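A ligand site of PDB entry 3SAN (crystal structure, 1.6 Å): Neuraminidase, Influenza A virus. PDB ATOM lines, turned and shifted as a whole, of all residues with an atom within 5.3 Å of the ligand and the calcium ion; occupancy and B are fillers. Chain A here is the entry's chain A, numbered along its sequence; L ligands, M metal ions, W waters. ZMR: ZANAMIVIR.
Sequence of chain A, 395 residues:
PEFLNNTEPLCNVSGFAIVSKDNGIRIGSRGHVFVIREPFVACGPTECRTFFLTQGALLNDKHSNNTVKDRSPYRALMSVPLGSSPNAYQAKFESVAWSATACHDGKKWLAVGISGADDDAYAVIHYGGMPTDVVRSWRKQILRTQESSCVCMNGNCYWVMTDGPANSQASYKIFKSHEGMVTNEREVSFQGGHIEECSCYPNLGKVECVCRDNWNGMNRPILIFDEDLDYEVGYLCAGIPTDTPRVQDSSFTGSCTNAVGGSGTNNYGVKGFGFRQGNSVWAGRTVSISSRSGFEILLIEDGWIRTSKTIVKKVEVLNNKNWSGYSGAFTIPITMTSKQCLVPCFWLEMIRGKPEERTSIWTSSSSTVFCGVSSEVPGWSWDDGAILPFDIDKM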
ATOM      1  N   ARG A  37       5.290 -21.005   3.466  1.00  0.00           N
ATOM      2  CA  ARG A  37       6.240 -20.518   2.469  1.00  0.00           C
ATOM      3  C   ARG A  37       6.164 -18.998   2.493  1.00  0.00           C
ATOM      4  O   ARG A  37       5.387 -18.439   3.272  1.00  0.00           O
ATOM      5  CB  ARG A  37       5.991 -21.082   1.063  1.00  0.00           C
ATOM      6  CG  ARG A  37       6.939 -22.231   0.687  1.00  0.00           C
ATOM      7  CD  ARG A  37       7.238 -22.252  -0.819  1.00  0.00           C
ATOM      8  NE  ARG A  37       7.925 -21.031  -1.206  1.00  0.00           N
ATOM      9  CZ  ARG A  37       7.857 -20.474  -2.419  1.00  0.00           C
ATOM     10  NH1 ARG A  37       7.137 -21.030  -3.387  1.00  0.00           N
ATOM     11  NH2 ARG A  37       8.529 -19.355  -2.654  1.00  0.00           N
ATOM     12  N   GLU A  38       6.974 -18.346   1.680  1.00  0.00           N
ATOM     13  CA  GLU A  38       6.975 -16.884   1.620  1.00  0.00           C
ATOM     14  C   GLU A  38       7.179 -16.223   2.990  1.00  0.00           C
ATOM     15  O   GLU A  38       6.395 -15.366   3.403  1.00  0.00           O
ATOM     16  CB  GLU A  38       5.681 -16.377   0.963  1.00  0.00           C
ATOM     17  CG  GLU A  38       5.471 -16.875  -0.487  1.00  0.00           C
ATOM     18  CD  GLU A  38       4.811 -18.244  -0.586  1.00  0.00           C
ATOM     19  OE1 GLU A  38       4.038 -18.631   0.316  1.00  0.00           O
ATOM     20  OE2 GLU A  38       5.064 -18.943  -1.593  1.00  0.00           O
ATOM     21  N   LEU A  53       3.481 -17.116   5.425  1.00  0.00           N
ATOM     22  CA  LEU A  53       2.177 -17.601   5.002  1.00  0.00           C
ATOM     23  C   LEU A  53       2.055 -19.075   5.335  1.00  0.00           C
ATOM     24  O   LEU A  53       2.718 -19.904   4.718  1.00  0.00           O
ATOM     25  CB  LEU A  53       1.989 -17.400   3.505  1.00  0.00           C
ATOM     26  CG  LEU A  53       2.043 -15.966   3.007  1.00  0.00           C
ATOM     27  CD1 LEU A  53       1.841 -15.928   1.494  1.00  0.00           C
ATOM     28  CD2 LEU A  53       1.011 -15.092   3.715  1.00  0.00           C
ATOM     29  N   ASP A  70      -0.254 -22.904  -4.268  1.00  0.00           N
ATOM     30  CA  ASP A  70       0.008 -21.529  -3.832  1.00  0.00           C
ATOM     31  C   ASP A  70      -1.118 -20.857  -3.045  1.00  0.00           C
ATOM     32  O   ASP A  70      -0.847 -20.051  -2.154  1.00  0.00           O
ATOM     33  CB  ASP A  70       0.369 -20.656  -5.022  1.00  0.00           C
ATOM     34  CG  ASP A  70       1.766 -20.904  -5.520  1.00  0.00           C
ATOM     35  OD1 ASP A  70       2.705 -20.811  -4.702  1.00  0.00           O
ATOM     36  OD2 ASP A  70       1.933 -21.192  -6.716  1.00  0.00           O
ATOM     37  N   ARG A  71      -2.368 -21.160  -3.384  1.00  0.00           N
ATOM     38  CA  ARG A  71      -3.464 -20.398  -2.812  1.00  0.00           C
ATOM     39  C   ARG A  71      -4.580 -21.312  -2.326  1.00  0.00           C
ATOM     40  O   ARG A  71      -4.913 -22.287  -2.984  1.00  0.00           O
ATOM     41  CB  ARG A  71      -3.993 -19.382  -3.841  1.00  0.00           C
ATOM     42  CG  ARG A  71      -2.903 -18.449  -4.381  1.00  0.00           C
ATOM     43  CD  ARG A  71      -3.398 -17.500  -5.467  1.00  0.00           C
ATOM     44  NE  ARG A  71      -3.878 -18.222  -6.658  1.00  0.00           N
ATOM     45  CZ  ARG A  71      -3.082 -18.733  -7.584  1.00  0.00           C
ATOM     46  NH1 ARG A  71      -1.756 -18.620  -7.475  1.00  0.00           N
ATOM     47  NH2 ARG A  71      -3.604 -19.374  -8.631  1.00  0.00           N
ATOM     48  N   ARG A  75      -4.732 -20.581   4.076  1.00  0.00           N
ATOM     49  CA  ARG A  75      -3.471 -19.868   4.289  1.00  0.00           C
ATOM     50  C   ARG A  75      -3.704 -18.601   5.102  1.00  0.00           C
ATOM     51  O   ARG A  75      -4.698 -17.884   4.904  1.00  0.00           O
ATOM     52  CB  ARG A  75      -2.774 -19.550   2.960  1.00  0.00           C
ATOM     53  CG  ARG A  75      -2.546 -20.778   2.092  1.00  0.00           C
ATOM     54  CD  ARG A  75      -1.381 -20.569   1.117  1.00  0.00           C
ATOM     55  NE  ARG A  75      -0.087 -20.539   1.808  1.00  0.00           N
ATOM     56  CZ  ARG A  75       1.085 -20.456   1.187  1.00  0.00           C
ATOM     57  NH1 ARG A  75       1.143 -20.374  -0.131  1.00  0.00           N
ATOM     58  NH2 ARG A  75       2.215 -20.437   1.891  1.00  0.00           N
ATOM     59  N   TRP A  98      -3.075 -15.442   1.244  1.00  0.00           N
ATOM     60  CA  TRP A  98      -2.178 -16.229   0.411  1.00  0.00           C
ATOM     61  C   TRP A  98      -1.142 -15.350  -0.313  1.00  0.00           C
ATOM     62  O   TRP A  98      -0.328 -15.837  -1.089  1.00  0.00           O
ATOM     63  CB  TRP A  98      -2.921 -17.187  -0.547  1.00  0.00           C
ATOM     64  CG  TRP A  98      -4.128 -16.676  -1.289  1.00  0.00           C
ATOM     65  CD1 TRP A  98      -5.429 -17.057  -1.097  1.00  0.00           C
ATOM     66  CD2 TRP A  98      -4.149 -15.729  -2.380  1.00  0.00           C
ATOM     67  NE1 TRP A  98      -6.259 -16.394  -1.984  1.00  0.00           N
ATOM     68  CE2 TRP A  98      -5.500 -15.579  -2.776  1.00  0.00           C
ATOM     69  CE3 TRP A  98      -3.156 -14.996  -3.042  1.00  0.00           C
ATOM     70  CZ2 TRP A  98      -5.880 -14.725  -3.807  1.00  0.00           C
ATOM     71  CZ3 TRP A  98      -3.544 -14.153  -4.069  1.00  0.00           C
ATOM     72  CH2 TRP A  98      -4.888 -14.019  -4.448  1.00  0.00           C
ATOM     73  N   SER A  99      -1.177 -14.056  -0.019  1.00  0.00           N
ATOM     74  CA  SER A  99      -0.153 -13.106  -0.445  1.00  0.00           C
ATOM     75  C   SER A  99      -0.196 -11.946   0.550  1.00  0.00           C
ATOM     76  O   SER A  99      -1.284 -11.590   1.012  1.00  0.00           O
ATOM     77  CB  SER A  99      -0.423 -12.600  -1.868  1.00  0.00           C
ATOM     78  OG  SER A  99       0.578 -11.675  -2.280  1.00  0.00           O
ATOM     79  N   ILE A 142      -5.705 -12.667  -9.887  1.00  0.00           N
ATOM     80  CA  ILE A 142      -4.752 -12.944  -8.810  1.00  0.00           C
ATOM     81  C   ILE A 142      -4.051 -11.694  -8.287  1.00  0.00           C
ATOM     82  O   ILE A 142      -2.837 -11.524  -8.439  1.00  0.00           O
ATOM     83  CB  ILE A 142      -3.730 -14.038  -9.196  1.00  0.00           C
ATOM     84  CG1 ILE A 142      -4.453 -15.224  -9.848  1.00  0.00           C
ATOM     85  CG2 ILE A 142      -2.936 -14.487  -7.965  1.00  0.00           C
ATOM     86  CD1 ILE A 142      -3.536 -16.329 -10.322  1.00  0.00           C
ATOM     87  N   LEU A 143      -4.831 -10.807  -7.678  1.00  0.00           N
ATOM     88  CA  LEU A 143      -4.275  -9.681  -6.955  1.00  0.00           C
ATOM     89  C   LEU A 143      -3.193 -10.209  -6.022  1.00  0.00           C
ATOM     90  O   LEU A 143      -3.390 -11.199  -5.325  1.00  0.00           O
ATOM     91  CB  LEU A 143      -5.372  -8.996  -6.148  1.00  0.00           C
ATOM     92  CG  LEU A 143      -4.941  -7.858  -5.225  1.00  0.00           C
ATOM     93  CD1 LEU A 143      -4.456  -6.653  -6.027  1.00  0.00           C
ATOM     94  CD2 LEU A 143      -6.109  -7.475  -4.325  1.00  0.00           C
ATOM     95  N   ARG A 144      -2.028  -9.569  -6.030  1.00  0.00           N
ATOM     96  CA  ARG A 144      -0.900 -10.093  -5.273  1.00  0.00           C
ATOM     97  C   ARG A 144       0.061  -8.987  -4.884  1.00  0.00           C
ATOM     98  O   ARG A 144       0.054  -7.899  -5.475  1.00  0.00           O
ATOM     99  CB  ARG A 144      -0.186 -11.188  -6.080  1.00  0.00           C
ATOM    100  CG  ARG A 144       0.233 -10.785  -7.480  1.00  0.00           C
ATOM    101  CD  ARG A 144       0.369 -12.031  -8.350  1.00  0.00           C
ATOM    102  NE  ARG A 144       0.907 -11.786  -9.694  1.00  0.00           N
ATOM    103  CZ  ARG A 144       0.174 -11.478 -10.760  1.00  0.00           C
ATOM    104  NH1 ARG A 144      -1.147 -11.336 -10.652  1.00  0.00           N
ATOM    105  NH2 ARG A 144       0.755 -11.310 -11.941  1.00  0.00           N
ATOM    106  N   GLU A 147       5.207 -10.035  -0.552  1.00  0.00           N
ATOM    107  CA  GLU A 147       5.760 -11.135   0.249  1.00  0.00           C
ATOM    108  C   GLU A 147       7.041 -10.700   0.952  1.00  0.00           C
ATOM    109  O   GLU A 147       7.976 -11.485   1.141  1.00  0.00           O
ATOM    110  CB  GLU A 147       6.015 -12.397  -0.585  1.00  0.00           C
ATOM    111  CG  GLU A 147       5.059 -12.618  -1.750  1.00  0.00           C
ATOM    112  CD  GLU A 147       3.623 -12.858  -1.331  1.00  0.00           C
ATOM    113  OE1 GLU A 147       3.325 -12.837  -0.115  1.00  0.00           O
ATOM    114  OE2 GLU A 147       2.774 -13.068  -2.220  1.00  0.00           O
ATOM    115  N   ALA A 166       0.428 -13.681 -15.279  1.00  0.00           N
ATOM    116  CA  ALA A 166       1.716 -14.044 -14.709  1.00  0.00           C
ATOM    117  C   ALA A 166       2.820 -13.990 -15.751  1.00  0.00           C
ATOM    118  O   ALA A 166       3.980 -13.792 -15.404  1.00  0.00           O
ATOM    119  CB  ALA A 166       1.640 -15.440 -14.102  1.00  0.00           C
ATOM    120  N   GLU A 196       6.570  -7.958  -9.960  1.00  0.00           N
ATOM    121  CA  GLU A 196       5.960  -8.792  -8.930  1.00  0.00           C
ATOM    122  C   GLU A 196       6.870  -8.815  -7.720  1.00  0.00           C
ATOM    123  O   GLU A 196       8.077  -8.613  -7.840  1.00  0.00           O
ATOM    124  CB  GLU A 196       5.802 -10.231  -9.405  1.00  0.00           C
ATOM    125  CG  GLU A 196       4.869 -10.399 -10.574  1.00  0.00           C
ATOM    126  CD  GLU A 196       4.587 -11.851 -10.872  1.00  0.00           C
ATOM    127  OE1 GLU A 196       5.529 -12.668 -10.746  1.00  0.00           O
ATOM    128  OE2 GLU A 196       3.437 -12.168 -11.242  1.00  0.00           O
ATOM    129  N   GLU A 197       6.271  -9.092  -6.560  1.00  0.00           N
ATOM    130  CA  GLU A 197       7.035  -9.434  -5.363  1.00  0.00           C
ATOM    131  C   GLU A 197       8.191  -8.470  -5.072  1.00  0.00           C
ATOM    132  O   GLU A 197       9.331  -8.878  -4.865  1.00  0.00           O
ATOM    133  CB  GLU A 197       7.534 -10.876  -5.472  1.00  0.00           C
ATOM    134  CG  GLU A 197       6.377 -11.869  -5.482  1.00  0.00           C
ATOM    135  CD  GLU A 197       6.789 -13.292  -5.774  1.00  0.00           C
ATOM    136  OE1 GLU A 197       7.885 -13.509  -6.339  1.00  0.00           O
ATOM    137  OE2 GLU A 197       5.996 -14.201  -5.460  1.00  0.00           O
ATOM    138  N   ARG A 212      10.613  -8.717  -9.207  1.00  0.00           N
ATOM    139  CA  ARG A 212      10.687  -9.906 -10.053  1.00  0.00           C
ATOM    140  C   ARG A 212       9.922  -9.661 -11.342  1.00  0.00           C
ATOM    141  O   ARG A 212       8.762  -9.237 -11.307  1.00  0.00           O
ATOM    142  CB  ARG A 212      10.077 -11.089  -9.308  1.00  0.00           C
ATOM    143  CG  ARG A 212       9.747 -12.316 -10.160  1.00  0.00           C
ATOM    144  CD  ARG A 212       9.019 -13.357  -9.291  1.00  0.00           C
ATOM    145  NE  ARG A 212       8.581 -14.546 -10.023  1.00  0.00           N
ATOM    146  CZ  ARG A 212       8.127 -15.651  -9.433  1.00  0.00           C
ATOM    147  NH1 ARG A 212       8.076 -15.736  -8.108  1.00  0.00           N
ATOM    148  NH2 ARG A 212       7.743 -16.699 -10.153  1.00  0.00           N
ATOM    149  N   ASP A 213      10.571  -9.900 -12.474  1.00  0.00           N
ATOM    150  CA  ASP A 213       9.904  -9.855 -13.772  1.00  0.00           C
ATOM    151  C   ASP A 213       9.623 -11.304 -14.143  1.00  0.00           C
ATOM    152  O   ASP A 213      10.544 -12.093 -14.262  1.00  0.00           O
ATOM    153  CB  ASP A 213      10.820  -9.170 -14.794  1.00  0.00           C
ATOM    154  CG  ASP A 213      10.233  -9.137 -16.190  1.00  0.00           C
ATOM    155  OD1 ASP A 213       9.723 -10.167 -16.664  1.00  0.00           O
ATOM    156  OD2 ASP A 213      10.304  -8.065 -16.835  1.00  0.00           O
ATOM    157  N   ASN A 214       8.346 -11.670 -14.288  1.00  0.00           N
ATOM    158  CA  ASN A 214       7.986 -13.072 -14.536  1.00  0.00           C
ATOM    159  C   ASN A 214       7.624 -13.289 -15.997  1.00  0.00           C
ATOM    160  O   ASN A 214       7.014 -14.307 -16.366  1.00  0.00           O
ATOM    161  CB  ASN A 214       6.815 -13.486 -13.643  1.00  0.00           C
ATOM    162  CG  ASN A 214       6.827 -14.968 -13.329  1.00  0.00           C
ATOM    163  OD1 ASN A 214       7.791 -15.491 -12.756  1.00  0.00           O
ATOM    164  ND2 ASN A 214       5.740 -15.653 -13.675  1.00  0.00           N
ATOM    165  N   TRP A 215       8.008 -12.333 -16.832  1.00  0.00           N
ATOM    166  CA  TRP A 215       7.627 -12.282 -18.236  1.00  0.00           C
ATOM    167  C   TRP A 215       8.883 -12.388 -19.094  1.00  0.00           C
ATOM    168  O   TRP A 215       9.433 -13.473 -19.271  1.00  0.00           O
ATOM    169  CB  TRP A 215       6.856 -10.986 -18.490  1.00  0.00           C
ATOM    170  CG  TRP A 215       6.252 -10.823 -19.866  1.00  0.00           C
ATOM    171  CD1 TRP A 215       6.090 -11.781 -20.817  1.00  0.00           C
ATOM    172  CD2 TRP A 215       5.718  -9.616 -20.415  1.00  0.00           C
ATOM    173  NE1 TRP A 215       5.509 -11.239 -21.935  1.00  0.00           N
ATOM    174  CE2 TRP A 215       5.265  -9.915 -21.713  1.00  0.00           C
ATOM    175  CE3 TRP A 215       5.587  -8.307 -19.934  1.00  0.00           C
ATOM    176  CZ2 TRP A 215       4.693  -8.951 -22.544  1.00  0.00           C
ATOM    177  CZ3 TRP A 215       5.014  -7.357 -20.755  1.00  0.00           C
ATOM    178  CH2 TRP A 215       4.574  -7.680 -22.045  1.00  0.00           C
ATOM    179  N   GLY A 217      11.965 -10.718 -18.598  1.00  0.00           N
ATOM    180  CA  GLY A 217      13.208 -10.246 -18.003  1.00  0.00           C
ATOM    181  C   GLY A 217      13.904 -11.187 -17.026  1.00  0.00           C
ATOM    182  O   GLY A 217      13.289 -11.657 -16.078  1.00  0.00           O
ATOM    183  N   MET A 218      15.195 -11.444 -17.262  1.00  0.00           N
ATOM    184  CA  MET A 218      16.021 -12.162 -16.304  1.00  0.00           C
ATOM    185  C   MET A 218      16.820 -11.136 -15.493  1.00  0.00           C
ATOM    186  O   MET A 218      17.526 -11.488 -14.547  1.00  0.00           O
ATOM    187  CB  MET A 218      16.971 -13.129 -17.008  1.00  0.00           C
ATOM    188  CG  MET A 218      18.147 -12.446 -17.693  1.00  0.00           C
ATOM    189  SD  MET A 218      19.298 -13.587 -18.498  1.00  0.00           S
ATOM    190  CE  MET A 218      18.546 -13.763 -20.109  1.00  0.00           C
ATOM    191  N   ASP A 243      18.005 -12.574 -11.593  1.00  0.00           N
ATOM    192  CA  ASP A 243      16.795 -13.378 -11.469  1.00  0.00           C
ATOM    193  C   ASP A 243      17.188 -14.849 -11.643  1.00  0.00           C
ATOM    194  O   ASP A 243      18.338 -15.159 -11.962  1.00  0.00           O
ATOM    195  CB  ASP A 243      15.761 -12.980 -12.524  1.00  0.00           C
ATOM    196  CG  ASP A 243      14.334 -13.406 -12.181  1.00  0.00           C
ATOM    197  OD1 ASP A 243      14.080 -13.967 -11.086  1.00  0.00           O
ATOM    198  OD2 ASP A 243      13.444 -13.160 -13.012  1.00  0.00           O
ATOM    199  N   PRO A 245      15.052 -18.192 -13.513  1.00  0.00           N
ATOM    200  CA  PRO A 245      16.233 -18.555 -14.317  1.00  0.00           C
ATOM    201  C   PRO A 245      16.906 -17.367 -15.020  1.00  0.00           C
ATOM    202  O   PRO A 245      16.293 -16.321 -15.231  1.00  0.00           O
ATOM    203  CB  PRO A 245      15.663 -19.513 -15.357  1.00  0.00           C
ATOM    204  CG  PRO A 245      14.248 -19.053 -15.536  1.00  0.00           C
ATOM    205  CD  PRO A 245      13.800 -18.600 -14.177  1.00  0.00           C
ATOM    206  N   THR A 265      14.856 -18.399 -20.457  1.00  0.00           N
ATOM    207  CA  THR A 265      14.664 -17.766 -19.156  1.00  0.00           C
ATOM    208  C   THR A 265      13.307 -17.069 -19.003  1.00  0.00           C
ATOM    209  O   THR A 265      12.964 -16.636 -17.914  1.00  0.00           O
ATOM    210  CB  THR A 265      15.760 -16.712 -18.876  1.00  0.00           C
ATOM    211  OG1 THR A 265      15.549 -15.570 -19.710  1.00  0.00           O
ATOM    212  CG2 THR A 265      17.145 -17.302 -19.135  1.00  0.00           C
ATOM    213  N   TYR A 268       9.347 -17.076 -16.035  1.00  0.00           N
ATOM    214  CA  TYR A 268       9.496 -17.455 -14.635  1.00  0.00           C
ATOM    215  C   TYR A 268      10.416 -16.472 -13.960  1.00  0.00           C
ATOM    216  O   TYR A 268      10.810 -15.468 -14.556  1.00  0.00           O
ATOM    217  CB  TYR A 268      10.024 -18.895 -14.497  1.00  0.00           C
ATOM    218  CG  TYR A 268       9.639 -19.566 -13.182  1.00  0.00           C
ATOM    219  CD1 TYR A 268       8.327 -19.531 -12.714  1.00  0.00           C
ATOM    220  CD2 TYR A 268      10.585 -20.260 -12.435  1.00  0.00           C
ATOM    221  CE1 TYR A 268       7.968 -20.161 -11.526  1.00  0.00           C
ATOM    222  CE2 TYR A 268      10.240 -20.891 -11.247  1.00  0.00           C
ATOM    223  CZ  TYR A 268       8.929 -20.829 -10.800  1.00  0.00           C
ATOM    224  OH  TYR A 268       8.571 -21.454  -9.626  1.00  0.00           O
ATOM    225  N   GLY A 269      10.735 -16.745 -12.705  1.00  0.00           N
ATOM    226  CA  GLY A 269      11.537 -15.826 -11.921  1.00  0.00           C
ATOM    227  C   GLY A 269      11.484 -16.276 -10.477  1.00  0.00           C
ATOM    228  O   GLY A 269      10.905 -17.310 -10.159  1.00  0.00           O
ATOM    229  N   ARG A 292      16.384 -23.026  -7.999  1.00  0.00           N
ATOM    230  CA  ARG A 292      16.451 -22.305  -6.734  1.00  0.00           C
ATOM    231  C   ARG A 292      17.361 -23.050  -5.767  1.00  0.00           C
ATOM    232  O   ARG A 292      16.902 -23.650  -4.789  1.00  0.00           O
ATOM    233  CB  ARG A 292      15.050 -22.102  -6.163  1.00  0.00           C
ATOM    234  CG  ARG A 292      14.179 -21.223  -7.062  1.00  0.00           C
ATOM    235  CD  ARG A 292      12.695 -21.332  -6.752  1.00  0.00           C
ATOM    236  NE  ARG A 292      11.946 -20.324  -7.508  1.00  0.00           N
ATOM    237  CZ  ARG A 292      10.671 -20.012  -7.283  1.00  0.00           C
ATOM    238  NH1 ARG A 292       9.994 -20.630  -6.327  1.00  0.00           N
ATOM    239  NH2 ARG A 292      10.082 -19.069  -8.017  1.00  0.00           N
ATOM    240  N   TYR A 326      12.961 -17.775  -2.204  1.00  0.00           N
ATOM    241  CA  TYR A 326      12.782 -16.325  -2.147  1.00  0.00           C
ATOM    242  C   TYR A 326      13.835 -15.648  -1.291  1.00  0.00           C
ATOM    243  O   TYR A 326      14.397 -16.257  -0.382  1.00  0.00           O
ATOM    244  CB  TYR A 326      11.401 -15.991  -1.591  1.00  0.00           C
ATOM    245  CG  TYR A 326      10.290 -16.089  -2.603  1.00  0.00           C
ATOM    246  CD1 TYR A 326      10.494 -16.716  -3.826  1.00  0.00           C
ATOM    247  CD2 TYR A 326       9.029 -15.570  -2.332  1.00  0.00           C
ATOM    248  CE1 TYR A 326       9.480 -16.802  -4.756  1.00  0.00           C
ATOM    249  CE2 TYR A 326       8.015 -15.656  -3.261  1.00  0.00           C
ATOM    250  CZ  TYR A 326       8.255 -16.277  -4.474  1.00  0.00           C
ATOM    251  OH  TYR A 326       7.248 -16.371  -5.413  1.00  0.00           O
HETATM  252  C1  ZMR L   1       6.794 -18.927  -6.792  1.00  0.00           C
HETATM  253  O1A ZMR L   1       7.166 -18.783  -7.877  1.00  0.00           O
HETATM  254  O1B ZMR L   1       7.262 -19.788  -5.909  1.00  0.00           O
HETATM  255  C2  ZMR L   1       5.516 -18.272  -6.485  1.00  0.00           C
HETATM  256  C3  ZMR L   1       4.942 -18.287  -5.068  1.00  0.00           C
HETATM  257  C4  ZMR L   1       3.680 -17.477  -4.851  1.00  0.00           C
HETATM  258  C5  ZMR L   1       3.017 -16.935  -6.091  1.00  0.00           C
HETATM  259  N5  ZMR L   1       2.013 -15.981  -5.759  1.00  0.00           N
HETATM  260  C10 ZMR L   1       0.630 -16.258  -5.811  1.00  0.00           C
HETATM  261  O10 ZMR L   1       0.201 -17.326  -5.885  1.00  0.00           O
HETATM  262  C11 ZMR L   1      -0.171 -15.088  -5.356  1.00  0.00           C
HETATM  263  C6  ZMR L   1       3.953 -16.531  -7.219  1.00  0.00           C
HETATM  264  O6  ZMR L   1       5.001 -17.429  -7.502  1.00  0.00           O
HETATM  265  C7  ZMR L   1       3.280 -16.289  -8.542  1.00  0.00           C
HETATM  266  O7  ZMR L   1       2.816 -17.460  -9.068  1.00  0.00           O
HETATM  267  C8  ZMR L   1       4.263 -15.627  -9.466  1.00  0.00           C
HETATM  268  O8  ZMR L   1       4.770 -14.481  -8.961  1.00  0.00           O
HETATM  269  C9  ZMR L   1       3.625 -15.422 -10.807  1.00  0.00           C
HETATM  270  O9  ZMR L   1       2.606 -14.526 -10.843  1.00  0.00           O
HETATM  271  NE  ZMR L   1       2.827 -18.033  -3.844  1.00  0.00           N
HETATM  272  CZ  ZMR L   1       2.077 -17.252  -2.941  1.00  0.00           C
HETATM  273  NH1 ZMR L   1       2.443 -16.033  -2.648  1.00  0.00           N
HETATM  274  NH2 ZMR L   1       1.164 -17.925  -2.279  1.00  0.00           N
HETATM  275 CA    CA M   1      12.233 -13.560 -15.019  1.00  0.00          CA
HETATM  276  O   HOH W   1      13.863 -15.278 -15.778  1.00  0.00           O
HETATM  277  O   HOH W   2      -0.063 -14.943 -10.603  1.00  0.00           O
HETATM  278  O   HOH W   3       0.082 -17.384  -9.719  1.00  0.00           O
HETATM  279  O   HOH W   4       3.468 -12.659  -7.300  1.00  0.00           O
HETATM  280  O   HOH W   5       5.988 -21.873  -8.877  1.00  0.00           O
HETATM  281  O   HOH W   6       4.911 -21.978  -5.878  1.00  0.00           O
HETATM  282  O   HOH W   7       3.502 -13.891  -4.597  1.00  0.00           O
HETATM  283  O   HOH W   8      11.476 -13.923 -17.316  1.00  0.00           O
HETATM  284  O   HOH W   9       5.027 -19.143  -9.794  1.00  0.00           O
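Residues that only touch the calcium ion: Gly 269. Five residues have an atom within 4 Å of the calcium ion: Asp 213, Gly 217, Asp 243, Tyr 268 and Gly 269. The nearest printed residue that does not touch the calcium ion is Met 218 (4.2 Å).
O1A of the ligand is in hydrogen-bond range of OH of Tyr 268, at 3.5 Å. An oxygen (O9) of the ligand sits at hydrogen-bond distance from the side-chain carboxylate of Glu 196 (2.5 Å). The side-chain hydroxyl (OH) of Tyr 326 sits close to an oxygen (O6) of the ligand (3.2 Å). O1B of the ligand is in salt-bridge range of NH1 of Arg 37 (2.8 Å). O of Trp 98 lies within hydrogen-bond range of NH2 of the ligand, 2.8 Å away. NH1 of Arg 71 lies within hydrogen-bond range of O10 of the ligand (2.8 Å). NH1 of Arg 292 lies within salt-bridge range of O1B of the ligand, at 2.9 Å. The backbone carbonyl oxygen of Asp 70 is in hydrogen-bond range of a nitrogen (NH2) of the ligand (2.9 Å). A nitrogen (NE) of the ligand lies within salt-bridge range of the side-chain carboxylate (OD1) of Asp 70 (2.9 Å). The side-chain carboxylate of Glu 147 lies within salt-bridge range of a nitrogen (NH1) of the ligand (3.0 Å). O1A of the ligand is in salt-bridge range of NH2 of Arg 212, at 3.1 Å. OE2 of Glu 38 lies within salt-bridge range of NE of the ligand (3.3 Å). The guanidinium group (NE) of Arg 144 sits at hydrogen-bond distance from an oxygen (O9) of the ligand (3.4 Å).
O of Asp 213 is bound to the calcium ion, at 2.4 Å. The calcium ion is bound by OD2 of Asp 243 (2.4 Å). O of Gly 217 binds the calcium ion (2.4 Å). O of Tyr 268 binds the calcium ion (2.4 Å). Water W8 binds the calcium ion (2.4 Å). Water W1 binds the calcium ion, at 2.5 Å. The calcium ion has six donor atoms within binding distance.
The side-chain carboxylate (OD1) of Asp 213 lies within hydrogen-bond range of the backbone NH (N) of Gly 217 (3.0 Å). The backbone NH (N) of Trp 215 is in hydrogen-bond range of the side-chain carboxylate (OD1) of Asp 213 (2.8 Å). The backbone NH (N) of Asp 243 sits close to the backbone carbonyl oxygen (O) of Met 218, 3.2 Å away. The guanidinium group (NH1) of Arg 212 lies within hydrogen-bond range of the side-chain hydroxyl (OH) of Tyr 326, 2.9 Å away. The guanidinium group (NH2) of Arg 292 is in hydrogen-bond range of the backbone carbonyl oxygen (O) of Gly 269. The guanidinium group of Arg 212 is in salt-bridge range of the side-chain carboxylate of Glu 197 (2.9 Å). The guanidinium group (NH2) of Arg 75 is in hydrogen-bond range of the backbone carbonyl oxygen (O) of Leu 53, at 2.9 Å. The backbone carbonyl oxygen (O) of Ala 166 is in hydrogen-bond range of the side-chain amide nitrogen (ND2) of Asn 214, 3.1 Å away.
NH1 of Arg 75 lies close to NH2 of the ligand. Ile 142 touches the ligand. CB of Ala 166 touches O9 of the ligand, at 3.5 Å. Glu 197 touches the ligand (OE2 to C6, 3.6 Å). Asn 214 touches the ligand. Within 4 Å of the ligand: Arg 37, Glu 38, Asp 70, Arg 71, Arg 75, Trp 98, Ile 142, Arg 144, Glu 147, Ala 166, Glu 196, Glu 197, Arg 212, Asn 214, Tyr 268, Arg 292 and Tyr 326.
Water W1 lies within hydrogen-bond range of O of Thr 265 and O of Pro 245. Water W2 bridges an oxygen (O9) of the ligand (2.7 Å) and the guanidinium group (NE) of Arg 144 (3.4 Å). Water W4 bridges an oxygen (O8) of the ligand (2.8 Å) and the side-chain carboxylate (OE2) of Glu 197 (3.5 Å). Water W7 lies within hydrogen-bond range of the side-chain carboxylate of Glu 147 (2.6 Å), the side-chain carboxylate of Glu 197 (2.7 Å) and a nitrogen (N5) of the ligand (2.8 Å). Water W6 lies within hydrogen-bond range of OD1 of Asp 70 (2.8 Å), O1B of the ligand (3.2 Å) and NH1 of Arg 37 (3.5 Å). Water W5 bridges OH of Tyr 268 (2.7 Å) and O1A of the ligand (3.5 Å).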
